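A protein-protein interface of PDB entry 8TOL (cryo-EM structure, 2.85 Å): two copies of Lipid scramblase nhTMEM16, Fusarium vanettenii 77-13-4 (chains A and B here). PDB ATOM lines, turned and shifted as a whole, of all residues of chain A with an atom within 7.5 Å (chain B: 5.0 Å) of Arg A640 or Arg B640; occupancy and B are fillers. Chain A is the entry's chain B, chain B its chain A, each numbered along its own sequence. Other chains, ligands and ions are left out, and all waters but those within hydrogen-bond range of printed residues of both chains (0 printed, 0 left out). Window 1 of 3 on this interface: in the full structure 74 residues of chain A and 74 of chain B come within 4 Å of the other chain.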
ATOM      1  N   LEU A  90      15.747  -9.747  -9.772  1.00  0.00           N
ATOM      2  CA  LEU A  90      14.600  -9.968 -10.641  1.00  0.00           C
ATOM      3  C   LEU A  90      13.329  -9.370 -10.048  1.00  0.00           C
ATOM      4  O   LEU A  90      12.473  -8.873 -10.787  1.00  0.00           O
ATOM      5  CB  LEU A  90      14.452 -11.467 -10.902  1.00  0.00           C
ATOM      6  CG  LEU A  90      13.338 -12.036 -11.776  1.00  0.00           C
ATOM      7  CD1 LEU A  90      13.782 -13.364 -12.341  1.00  0.00           C
ATOM      8  CD2 LEU A  90      12.095 -12.245 -10.950  1.00  0.00           C
ATOM      9  N   GLY A  92      13.317  -6.749  -8.113  1.00  0.00           N
ATOM     10  CA  GLY A  92      13.506  -5.323  -7.970  1.00  0.00           C
ATOM     11  C   GLY A  92      13.954  -4.847  -6.607  1.00  0.00           C
ATOM     12  O   GLY A  92      14.112  -3.635  -6.421  1.00  0.00           O
ATOM     13  N   VAL A  95      18.916  -3.129  -7.443  1.00  0.00           N
ATOM     14  CA  VAL A  95      18.963  -2.541  -8.778  1.00  0.00           C
ATOM     15  C   VAL A  95      20.294  -2.755  -9.474  1.00  0.00           C
ATOM     16  O   VAL A  95      20.462  -2.287 -10.611  1.00  0.00           O
ATOM     17  CB  VAL A  95      18.628  -1.036  -8.741  1.00  0.00           C
ATOM     18  CG1 VAL A  95      17.123  -0.835  -8.719  1.00  0.00           C
ATOM     19  CG2 VAL A  95      19.270  -0.388  -7.534  1.00  0.00           C
ATOM     20  N   ARG A 250      14.570  -3.191  -1.047  1.00  0.00           N
ATOM     21  CA  ARG A 250      13.449  -2.351  -1.449  1.00  0.00           C
ATOM     22  C   ARG A 250      12.229  -3.231  -1.656  1.00  0.00           C
ATOM     23  O   ARG A 250      12.237  -4.110  -2.524  1.00  0.00           O
ATOM     24  CB  ARG A 250      13.771  -1.572  -2.724  1.00  0.00           C
ATOM     25  CG  ARG A 250      14.561  -0.308  -2.480  1.00  0.00           C
ATOM     26  CD  ARG A 250      13.644   0.862  -2.183  1.00  0.00           C
ATOM     27  NE  ARG A 250      13.112   1.462  -3.400  1.00  0.00           N
ATOM     28  CZ  ARG A 250      12.071   2.281  -3.436  1.00  0.00           C
ATOM     29  NH1 ARG A 250      11.423   2.624  -2.335  1.00  0.00           N
ATOM     30  NH2 ARG A 250      11.670   2.769  -4.605  1.00  0.00           N
ATOM     31  N   ILE A 272       1.782 -10.446 -11.067  1.00  0.00           N
ATOM     32  CA  ILE A 272       3.112  -9.888 -11.284  1.00  0.00           C
ATOM     33  C   ILE A 272       4.099 -10.966 -11.722  1.00  0.00           C
ATOM     34  O   ILE A 272       4.692 -10.877 -12.799  1.00  0.00           O
ATOM     35  CB  ILE A 272       3.615  -9.147 -10.025  1.00  0.00           C
ATOM     36  CG1 ILE A 272       2.882  -7.815  -9.866  1.00  0.00           C
ATOM     37  CG2 ILE A 272       5.115  -8.916 -10.105  1.00  0.00           C
ATOM     38  CD1 ILE A 272       3.374  -6.983  -8.704  1.00  0.00           C
ATOM     39  N   LEU A 633      16.791   7.310  -5.186  1.00  0.00           N
ATOM     40  CA  LEU A 633      15.847   7.197  -6.294  1.00  0.00           C
ATOM     41  C   LEU A 633      16.525   7.496  -7.624  1.00  0.00           C
ATOM     42  O   LEU A 633      16.238   6.844  -8.633  1.00  0.00           O
ATOM     43  CB  LEU A 633      14.660   8.131  -6.075  1.00  0.00           C
ATOM     44  CG  LEU A 633      13.692   7.738  -4.959  1.00  0.00           C
ATOM     45  CD1 LEU A 633      12.565   8.749  -4.847  1.00  0.00           C
ATOM     46  CD2 LEU A 633      13.141   6.343  -5.199  1.00  0.00           C
ATOM     47  N   GLN A 634      17.425   8.481  -7.645  1.00  0.00           N
ATOM     48  CA  GLN A 634      18.143   8.793  -8.875  1.00  0.00           C
ATOM     49  C   GLN A 634      19.001   7.619  -9.326  1.00  0.00           C
ATOM     50  O   GLN A 634      19.054   7.303 -10.517  1.00  0.00           O
ATOM     51  CB  GLN A 634      19.003  10.044  -8.683  1.00  0.00           C
ATOM     52  CG  GLN A 634      18.225  11.297  -8.300  1.00  0.00           C
ATOM     53  CD  GLN A 634      17.319  11.807  -9.408  1.00  0.00           C
ATOM     54  OE1 GLN A 634      17.336  11.302 -10.530  1.00  0.00           O
ATOM     55  NE2 GLN A 634      16.519  12.819  -9.093  1.00  0.00           N
ATOM     56  N   LYS A 635      19.674   6.952  -8.386  1.00  0.00           N
ATOM     57  CA  LYS A 635      20.510   5.812  -8.746  1.00  0.00           C
ATOM     58  C   LYS A 635      19.657   4.642  -9.222  1.00  0.00           C
ATOM     59  O   LYS A 635      20.025   3.941 -10.174  1.00  0.00           O
ATOM     60  CB  LYS A 635      21.397   5.429  -7.554  1.00  0.00           C
ATOM     61  CG  LYS A 635      22.172   4.107  -7.645  1.00  0.00           C
ATOM     62  CD  LYS A 635      21.357   2.877  -7.266  1.00  0.00           C
ATOM     63  CE  LYS A 635      22.199   1.617  -7.347  1.00  0.00           C
ATOM     64  NZ  LYS A 635      23.182   1.532  -6.235  1.00  0.00           N
ATOM     65  N   GLU A 636      18.514   4.412  -8.572  1.00  0.00           N
ATOM     66  CA  GLU A 636      17.615   3.355  -9.027  1.00  0.00           C
ATOM     67  C   GLU A 636      17.104   3.635 -10.436  1.00  0.00           C
ATOM     68  O   GLU A 636      17.059   2.736 -11.285  1.00  0.00           O
ATOM     69  CB  GLU A 636      16.449   3.207  -8.052  1.00  0.00           C
ATOM     70  CG  GLU A 636      15.292   2.385  -8.584  1.00  0.00           C
ATOM     71  CD  GLU A 636      14.146   2.292  -7.599  1.00  0.00           C
ATOM     72  OE1 GLU A 636      13.319   3.227  -7.559  1.00  0.00           O
ATOM     73  OE2 GLU A 636      14.072   1.287  -6.863  1.00  0.00           O
ATOM     74  N   ARG A 637      16.727   4.888 -10.705  1.00  0.00           N
ATOM     75  CA  ARG A 637      16.268   5.255 -12.039  1.00  0.00           C
ATOM     76  C   ARG A 637      17.385   5.137 -13.067  1.00  0.00           C
ATOM     77  O   ARG A 637      17.130   4.751 -14.209  1.00  0.00           O
ATOM     78  CB  ARG A 637      15.708   6.673 -12.028  1.00  0.00           C
ATOM     79  CG  ARG A 637      14.433   6.839 -12.830  1.00  0.00           C
ATOM     80  CD  ARG A 637      13.218   6.753 -11.925  1.00  0.00           C
ATOM     81  NE  ARG A 637      13.379   7.561 -10.722  1.00  0.00           N
ATOM     82  CZ  ARG A 637      13.328   8.886 -10.693  1.00  0.00           C
ATOM     83  NH1 ARG A 637      13.109   9.596 -11.787  1.00  0.00           N
ATOM     84  NH2 ARG A 637      13.501   9.516  -9.534  1.00  0.00           N
ATOM     85  N   LYS A 638      18.618   5.477 -12.691  1.00  0.00           N
ATOM     86  CA  LYS A 638      19.742   5.315 -13.605  1.00  0.00           C
ATOM     87  C   LYS A 638      19.983   3.847 -13.926  1.00  0.00           C
ATOM     88  O   LYS A 638      20.277   3.499 -15.075  1.00  0.00           O
ATOM     89  CB  LYS A 638      21.000   5.948 -13.012  1.00  0.00           C
ATOM     90  CG  LYS A 638      22.210   5.886 -13.926  1.00  0.00           C
ATOM     91  CD  LYS A 638      23.456   6.399 -13.228  1.00  0.00           C
ATOM     92  CE  LYS A 638      24.437   6.997 -14.222  1.00  0.00           C
ATOM     93  NZ  LYS A 638      25.578   7.666 -13.541  1.00  0.00           N
ATOM     94  N   GLU A 639      19.872   2.973 -12.925  1.00  0.00           N
ATOM     95  CA  GLU A 639      20.006   1.541 -13.181  1.00  0.00           C
ATOM     96  C   GLU A 639      18.905   1.049 -14.111  1.00  0.00           C
ATOM     97  O   GLU A 639      19.159   0.245 -15.020  1.00  0.00           O
ATOM     98  CB  GLU A 639      19.985   0.767 -11.864  1.00  0.00           C
ATOM     99  N   ARG A 640      17.674   1.519 -13.899  1.00  0.00           N
ATOM    100  CA  ARG A 640      16.586   1.157 -14.803  1.00  0.00           C
ATOM    101  C   ARG A 640      16.860   1.653 -16.216  1.00  0.00           C
ATOM    102  O   ARG A 640      16.628   0.932 -17.190  1.00  0.00           O
ATOM    103  CB  ARG A 640      15.262   1.720 -14.288  1.00  0.00           C
ATOM    104  CG  ARG A 640      14.052   0.899 -14.692  1.00  0.00           C
ATOM    105  CD  ARG A 640      13.159   0.608 -13.502  1.00  0.00           C
ATOM    106  NE  ARG A 640      12.952   1.793 -12.677  1.00  0.00           N
ATOM    107  CZ  ARG A 640      12.216   1.818 -11.575  1.00  0.00           C
ATOM    108  NH1 ARG A 640      11.604   0.735 -11.128  1.00  0.00           N
ATOM    109  NH2 ARG A 640      12.093   2.960 -10.904  1.00  0.00           N
ATOM    110  N   PHE A 641      17.362   2.882 -16.345  1.00  0.00           N
ATOM    111  CA  PHE A 641      17.702   3.421 -17.656  1.00  0.00           C
ATOM    112  C   PHE A 641      18.761   2.570 -18.340  1.00  0.00           C
ATOM    113  O   PHE A 641      18.658   2.283 -19.539  1.00  0.00           O
ATOM    114  CB  PHE A 641      18.188   4.863 -17.501  1.00  0.00           C
ATOM    115  CG  PHE A 641      18.646   5.501 -18.783  1.00  0.00           C
ATOM    116  CD1 PHE A 641      17.759   6.205 -19.576  1.00  0.00           C
ATOM    117  CD2 PHE A 641      19.968   5.413 -19.183  1.00  0.00           C
ATOM    118  CE1 PHE A 641      18.183   6.800 -20.745  1.00  0.00           C
ATOM    119  CE2 PHE A 641      20.394   6.000 -20.355  1.00  0.00           C
ATOM    120  CZ  PHE A 641      19.499   6.693 -21.138  1.00  0.00           C
ATOM    121  N   GLN A 642      19.790   2.169 -17.597  1.00  0.00           N
ATOM    122  CA  GLN A 642      20.861   1.370 -18.181  1.00  0.00           C
ATOM    123  C   GLN A 642      20.351   0.004 -18.626  1.00  0.00           C
ATOM    124  O   GLN A 642      20.700  -0.473 -19.711  1.00  0.00           O
ATOM    125  CB  GLN A 642      22.008   1.224 -17.184  1.00  0.00           C
ATOM    126  CG  GLN A 642      22.731   2.526 -16.892  1.00  0.00           C
ATOM    127  CD  GLN A 642      23.866   2.790 -17.856  1.00  0.00           C
ATOM    128  OE1 GLN A 642      24.317   1.889 -18.563  1.00  0.00           O
ATOM    129  NE2 GLN A 642      24.334   4.031 -17.892  1.00  0.00           N
ATOM    130  N   THR A 643      19.517  -0.639 -17.807  1.00  0.00           N
ATOM    131  CA  THR A 643      19.008  -1.948 -18.202  1.00  0.00           C
ATOM    132  C   THR A 643      17.980  -1.853 -19.323  1.00  0.00           C
ATOM    133  O   THR A 643      17.784  -2.833 -20.048  1.00  0.00           O
ATOM    134  CB  THR A 643      18.411  -2.693 -17.004  1.00  0.00           C
ATOM    135  OG1 THR A 643      18.106  -4.039 -17.387  1.00  0.00           O
ATOM    136  CG2 THR A 643      17.139  -2.029 -16.526  1.00  0.00           C
ATOM    137  N   LYS A 644      17.325  -0.701 -19.485  1.00  0.00           N
ATOM    138  CA  LYS A 644      16.457  -0.504 -20.642  1.00  0.00           C
ATOM    139  C   LYS A 644      17.279  -0.284 -21.906  1.00  0.00           C
ATOM    140  O   LYS A 644      16.950  -0.825 -22.967  1.00  0.00           O
ATOM    141  CB  LYS A 644      15.528   0.689 -20.410  1.00  0.00           C
ATOM    142  CG  LYS A 644      14.516   0.513 -19.287  1.00  0.00           C
ATOM    143  CD  LYS A 644      13.612  -0.681 -19.479  1.00  0.00           C
ATOM    144  CE  LYS A 644      12.732  -0.506 -20.691  1.00  0.00           C
ATOM    145  NZ  LYS A 644      11.497  -1.325 -20.570  1.00  0.00           N
ATOM    146  N   LYS A 645      18.351   0.503 -21.804  1.00  0.00           N
ATOM    147  CA  LYS A 645      19.176   0.841 -22.955  1.00  0.00           C
ATOM    148  C   LYS A 645      20.087  -0.298 -23.387  1.00  0.00           C
ATOM    149  O   LYS A 645      20.537  -0.309 -24.538  1.00  0.00           O
ATOM    150  CB  LYS A 645      20.020   2.078 -22.643  1.00  0.00           C
ATOM    151  CG  LYS A 645      20.493   2.840 -23.864  1.00  0.00           C
ATOM    152  CD  LYS A 645      21.364   4.018 -23.465  1.00  0.00           C
ATOM    153  CE  LYS A 645      21.587   4.962 -24.632  1.00  0.00           C
ATOM    154  NZ  LYS A 645      22.297   6.200 -24.212  1.00  0.00           N
ATOM    155  N   ARG A 646      20.374  -1.247 -22.494  1.00  0.00           N
ATOM    156  CA  ARG A 646      21.253  -2.353 -22.855  1.00  0.00           C
ATOM    157  C   ARG A 646      20.658  -3.204 -23.970  1.00  0.00           C
ATOM    158  O   ARG A 646      21.399  -3.758 -24.790  1.00  0.00           O
ATOM    159  CB  ARG A 646      21.546  -3.206 -21.621  1.00  0.00           C
ATOM    160  CG  ARG A 646      22.371  -4.455 -21.890  1.00  0.00           C
ATOM    161  CD  ARG A 646      23.077  -4.970 -20.635  1.00  0.00           C
ATOM    162  NE  ARG A 646      22.552  -4.399 -19.399  1.00  0.00           N
ATOM    163  CZ  ARG A 646      23.106  -3.388 -18.743  1.00  0.00           C
ATOM    164  NH1 ARG A 646      24.207  -2.800 -19.181  1.00  0.00           N
ATOM    165  NH2 ARG A 646      22.538  -2.952 -17.622  1.00  0.00           N
ATOM    166  N   GLU B 636       1.963  -2.573 -15.153  1.00  0.00           N
ATOM    167  CA  GLU B 636       3.304  -2.012 -15.286  1.00  0.00           C
ATOM    168  C   GLU B 636       4.337  -2.881 -14.575  1.00  0.00           C
ATOM    169  O   GLU B 636       5.421  -3.145 -15.112  1.00  0.00           O
ATOM    170  CB  GLU B 636       3.331  -0.587 -14.738  1.00  0.00           C
ATOM    171  CG  GLU B 636       4.723  -0.031 -14.518  1.00  0.00           C
ATOM    172  CD  GLU B 636       4.703   1.370 -13.942  1.00  0.00           C
ATOM    173  OE1 GLU B 636       4.574   1.503 -12.707  1.00  0.00           O
ATOM    174  OE2 GLU B 636       4.813   2.337 -14.724  1.00  0.00           O
ATOM    175  N   ARG B 637       4.009  -3.346 -13.368  1.00  0.00           N
ATOM    176  CA  ARG B 637       4.916  -4.220 -12.637  1.00  0.00           C
ATOM    177  C   ARG B 637       5.097  -5.556 -13.343  1.00  0.00           C
ATOM    178  O   ARG B 637       6.195  -6.115 -13.327  1.00  0.00           O
ATOM    179  CB  ARG B 637       4.404  -4.438 -11.217  1.00  0.00           C
ATOM    180  CG  ARG B 637       5.484  -4.389 -10.156  1.00  0.00           C
ATOM    181  CD  ARG B 637       5.549  -3.013  -9.521  1.00  0.00           C
ATOM    182  NE  ARG B 637       4.223  -2.517  -9.169  1.00  0.00           N
ATOM    183  CZ  ARG B 637       3.493  -2.968  -8.159  1.00  0.00           C
ATOM    184  NH1 ARG B 637       3.932  -3.926  -7.361  1.00  0.00           N
ATOM    185  NH2 ARG B 637       2.291  -2.442  -7.943  1.00  0.00           N
ATOM    186  N   LYS B 638       4.037  -6.088 -13.952  1.00  0.00           N
ATOM    187  CA  LYS B 638       4.164  -7.328 -14.710  1.00  0.00           C
ATOM    188  C   LYS B 638       5.071  -7.144 -15.918  1.00  0.00           C
ATOM    189  O   LYS B 638       5.875  -8.027 -16.237  1.00  0.00           O
ATOM    190  CB  LYS B 638       2.785  -7.823 -15.144  1.00  0.00           C
ATOM    191  CG  LYS B 638       2.813  -9.149 -15.884  1.00  0.00           C
ATOM    192  CD  LYS B 638       1.438  -9.515 -16.411  1.00  0.00           C
ATOM    193  CE  LYS B 638       1.267 -11.022 -16.502  1.00  0.00           C
ATOM    194  NZ  LYS B 638      -0.131 -11.402 -16.842  1.00  0.00           N
ATOM    195  N   GLU B 639       4.951  -6.009 -16.609  1.00  0.00           N
ATOM    196  CA  GLU B 639       5.849  -5.731 -17.726  1.00  0.00           C
ATOM    197  C   GLU B 639       7.292  -5.625 -17.254  1.00  0.00           C
ATOM    198  O   GLU B 639       8.211  -6.136 -17.910  1.00  0.00           O
ATOM    199  CB  GLU B 639       5.420  -4.449 -18.439  1.00  0.00           C
ATOM    200  N   ARG B 640       7.512  -4.964 -16.115  1.00  0.00           N
ATOM    201  CA  ARG B 640       8.859  -4.895 -15.557  1.00  0.00           C
ATOM    202  C   ARG B 640       9.379  -6.283 -15.206  1.00  0.00           C
ATOM    203  O   ARG B 640      10.540  -6.605 -15.472  1.00  0.00           O
ATOM    204  CB  ARG B 640       8.875  -3.993 -14.324  1.00  0.00           C
ATOM    205  CG  ARG B 640      10.209  -3.312 -14.082  1.00  0.00           C
ATOM    206  CD  ARG B 640      10.035  -1.825 -13.845  1.00  0.00           C
ATOM    207  NE  ARG B 640       8.937  -1.547 -12.928  1.00  0.00           N
ATOM    208  CZ  ARG B 640       8.566  -0.331 -12.551  1.00  0.00           C
ATOM    209  NH1 ARG B 640       9.183   0.749 -12.998  1.00  0.00           N
ATOM    210  NH2 ARG B 640       7.550  -0.198 -11.702  1.00  0.00           N
ATOM    211  N   PHE B 641       8.528  -7.121 -14.614  1.00  0.00           N
ATOM    212  CA  PHE B 641       8.922  -8.486 -14.287  1.00  0.00           C
ATOM    213  C   PHE B 641       9.312  -9.258 -15.538  1.00  0.00           C
ATOM    214  O   PHE B 641      10.315  -9.981 -15.543  1.00  0.00           O
ATOM    215  CB  PHE B 641       7.773  -9.187 -13.559  1.00  0.00           C
ATOM    216  CG  PHE B 641       8.034 -10.632 -13.241  1.00  0.00           C
ATOM    217  CD1 PHE B 641       8.613 -10.995 -12.041  1.00  0.00           C
ATOM    218  CD2 PHE B 641       7.679 -11.628 -14.136  1.00  0.00           C
ATOM    219  CE1 PHE B 641       8.841 -12.322 -11.744  1.00  0.00           C
ATOM    220  CE2 PHE B 641       7.913 -12.955 -13.845  1.00  0.00           C
ATOM    221  CZ  PHE B 641       8.495 -13.303 -12.649  1.00  0.00           C
ATOM    222  N   GLN B 642       8.525  -9.125 -16.604  1.00  0.00           N
ATOM    223  CA  GLN B 642       8.814  -9.848 -17.836  1.00  0.00           C
ATOM    224  C   GLN B 642      10.124  -9.380 -18.457  1.00  0.00           C
ATOM    225  O   GLN B 642      10.930 -10.197 -18.915  1.00  0.00           O
ATOM    226  CB  GLN B 642       7.658  -9.689 -18.821  1.00  0.00           C
ATOM    227  CG  GLN B 642       6.376 -10.364 -18.369  1.00  0.00           C
ATOM    228  CD  GLN B 642       6.293 -11.808 -18.813  1.00  0.00           C
ATOM    229  OE1 GLN B 642       7.033 -12.242 -19.695  1.00  0.00           O
ATOM    230  NE2 GLN B 642       5.392 -12.565 -18.200  1.00  0.00           N
ATOM    231  N   THR B 643      10.363  -8.066 -18.476  1.00  0.00           N
ATOM    232  CA  THR B 643      11.608  -7.582 -19.062  1.00  0.00           C
ATOM    233  C   THR B 643      12.815  -7.881 -18.180  1.00  0.00           C
ATOM    234  O   THR B 643      13.937  -7.939 -18.690  1.00  0.00           O
ATOM    235  CB  THR B 643      11.533  -6.082 -19.358  1.00  0.00           C
ATOM    236  OG1 THR B 643      12.688  -5.687 -20.107  1.00  0.00           O
ATOM    237  CG2 THR B 643      11.490  -5.274 -18.080  1.00  0.00           C
ATOM    238  N   LYS B 644      12.612  -8.074 -16.875  1.00  0.00           N
ATOM    239  CA  LYS B 644      13.704  -8.527 -16.019  1.00  0.00           C
ATOM    240  C   LYS B 644      14.002 -10.002 -16.252  1.00  0.00           C
ATOM    241  O   LYS B 644      15.169 -10.403 -16.311  1.00  0.00           O
ATOM    242  CB  LYS B 644      13.358  -8.292 -14.547  1.00  0.00           C
ATOM    243  CG  LYS B 644      13.224  -6.831 -14.139  1.00  0.00           C
ATOM    244  CD  LYS B 644      14.471  -6.021 -14.401  1.00  0.00           C
ATOM    245  CE  LYS B 644      15.618  -6.499 -13.547  1.00  0.00           C
ATOM    246  NZ  LYS B 644      16.617  -5.416 -13.349  1.00  0.00           N
ATOM    247  N   LYS B 645      12.956 -10.817 -16.392  1.00  0.00           N
ATOM    248  CA  LYS B 645      13.112 -12.257 -16.554  1.00  0.00           C
ATOM    249  C   LYS B 645      13.570 -12.650 -17.949  1.00  0.00           C
ATOM    250  O   LYS B 645      14.109 -13.748 -18.122  1.00  0.00           O
ATOM    251  CB  LYS B 645      11.792 -12.961 -16.234  1.00  0.00           C
ATOM    252  CG  LYS B 645      11.937 -14.417 -15.840  1.00  0.00           C
ATOM    253  CD  LYS B 645      10.578 -15.048 -15.593  1.00  0.00           C
ATOM    254  CE  LYS B 645      10.712 -16.395 -14.904  1.00  0.00           C
ATOM    255  NZ  LYS B 645       9.387 -16.946 -14.507  1.00  0.00           N
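The guanidinium group of Arg A640 lies close to the guanidinium group of Arg B640 (3.1 Å).
The side-chain carboxylate (OE1) of Glu B636 lies within salt-bridge range of the guanidinium group (NH2) of Arg B640 (3.6 Å). The side-chain carboxylate (OE1) of Glu A636 lies within salt-bridge range of the guanidinium group (NH2) of Arg A640 (3.6 Å).
Among the printed residues, merely in contact across the chains: Leu A90 with Phe B641 (3.4 Å), Ile A272 with Phe B641 (3.4 Å), Ile A272 with Arg B637 (3.4 Å) and Leu A90 with Lys B644 (3.9 Å).
Of the printed residues of chain B, Ile A272 touches Arg B637 (3.4 Å) and Phe B641 (3.4 Å). Arg A637 touches none of the printed residues of chain B. Arg A640 touches one residue of chain B. Glu B636 touches none of the printed residues of chain A. No residue of chain A comes within 4 Å of Glu B639. Arg B640 touches one residue of chain A. Printed residues of chain A within 4 Å of Phe B641: Leu A90 (3.4 Å) and Ile A272 (3.4 Å). The nearest printed residue of chain B that does not touch Arg A640 is Lys B644 (6.7 Å). The nearest residue of chain A that does not touch Arg B640 is Leu A90 (5.6 Å).
Of the 19 printed residues of chain A, 3 touch a printed residue of chain B. Hydrophobic or aromatic side chains of chain A within 4 Å of the printed part of chain B: Leu A90 and Ile A272. Of the 10 printed residues of chain B, 4 touch a printed residue of chain A. Printed residues of chain B that touch a printed residue of chain A: Arg B637, Arg B640, Phe B641 and Lys B644. Among the printed residues, no Asp or Glu carboxylate lies within 4 Å of a Lys or Arg side-chain nitrogen of the other chain.
Arg A640 touches its own counterpart, Arg B640. Positions printed for both chains: 636, 637, 638, 639, 640, 641, 642, 643, 644 and 645.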
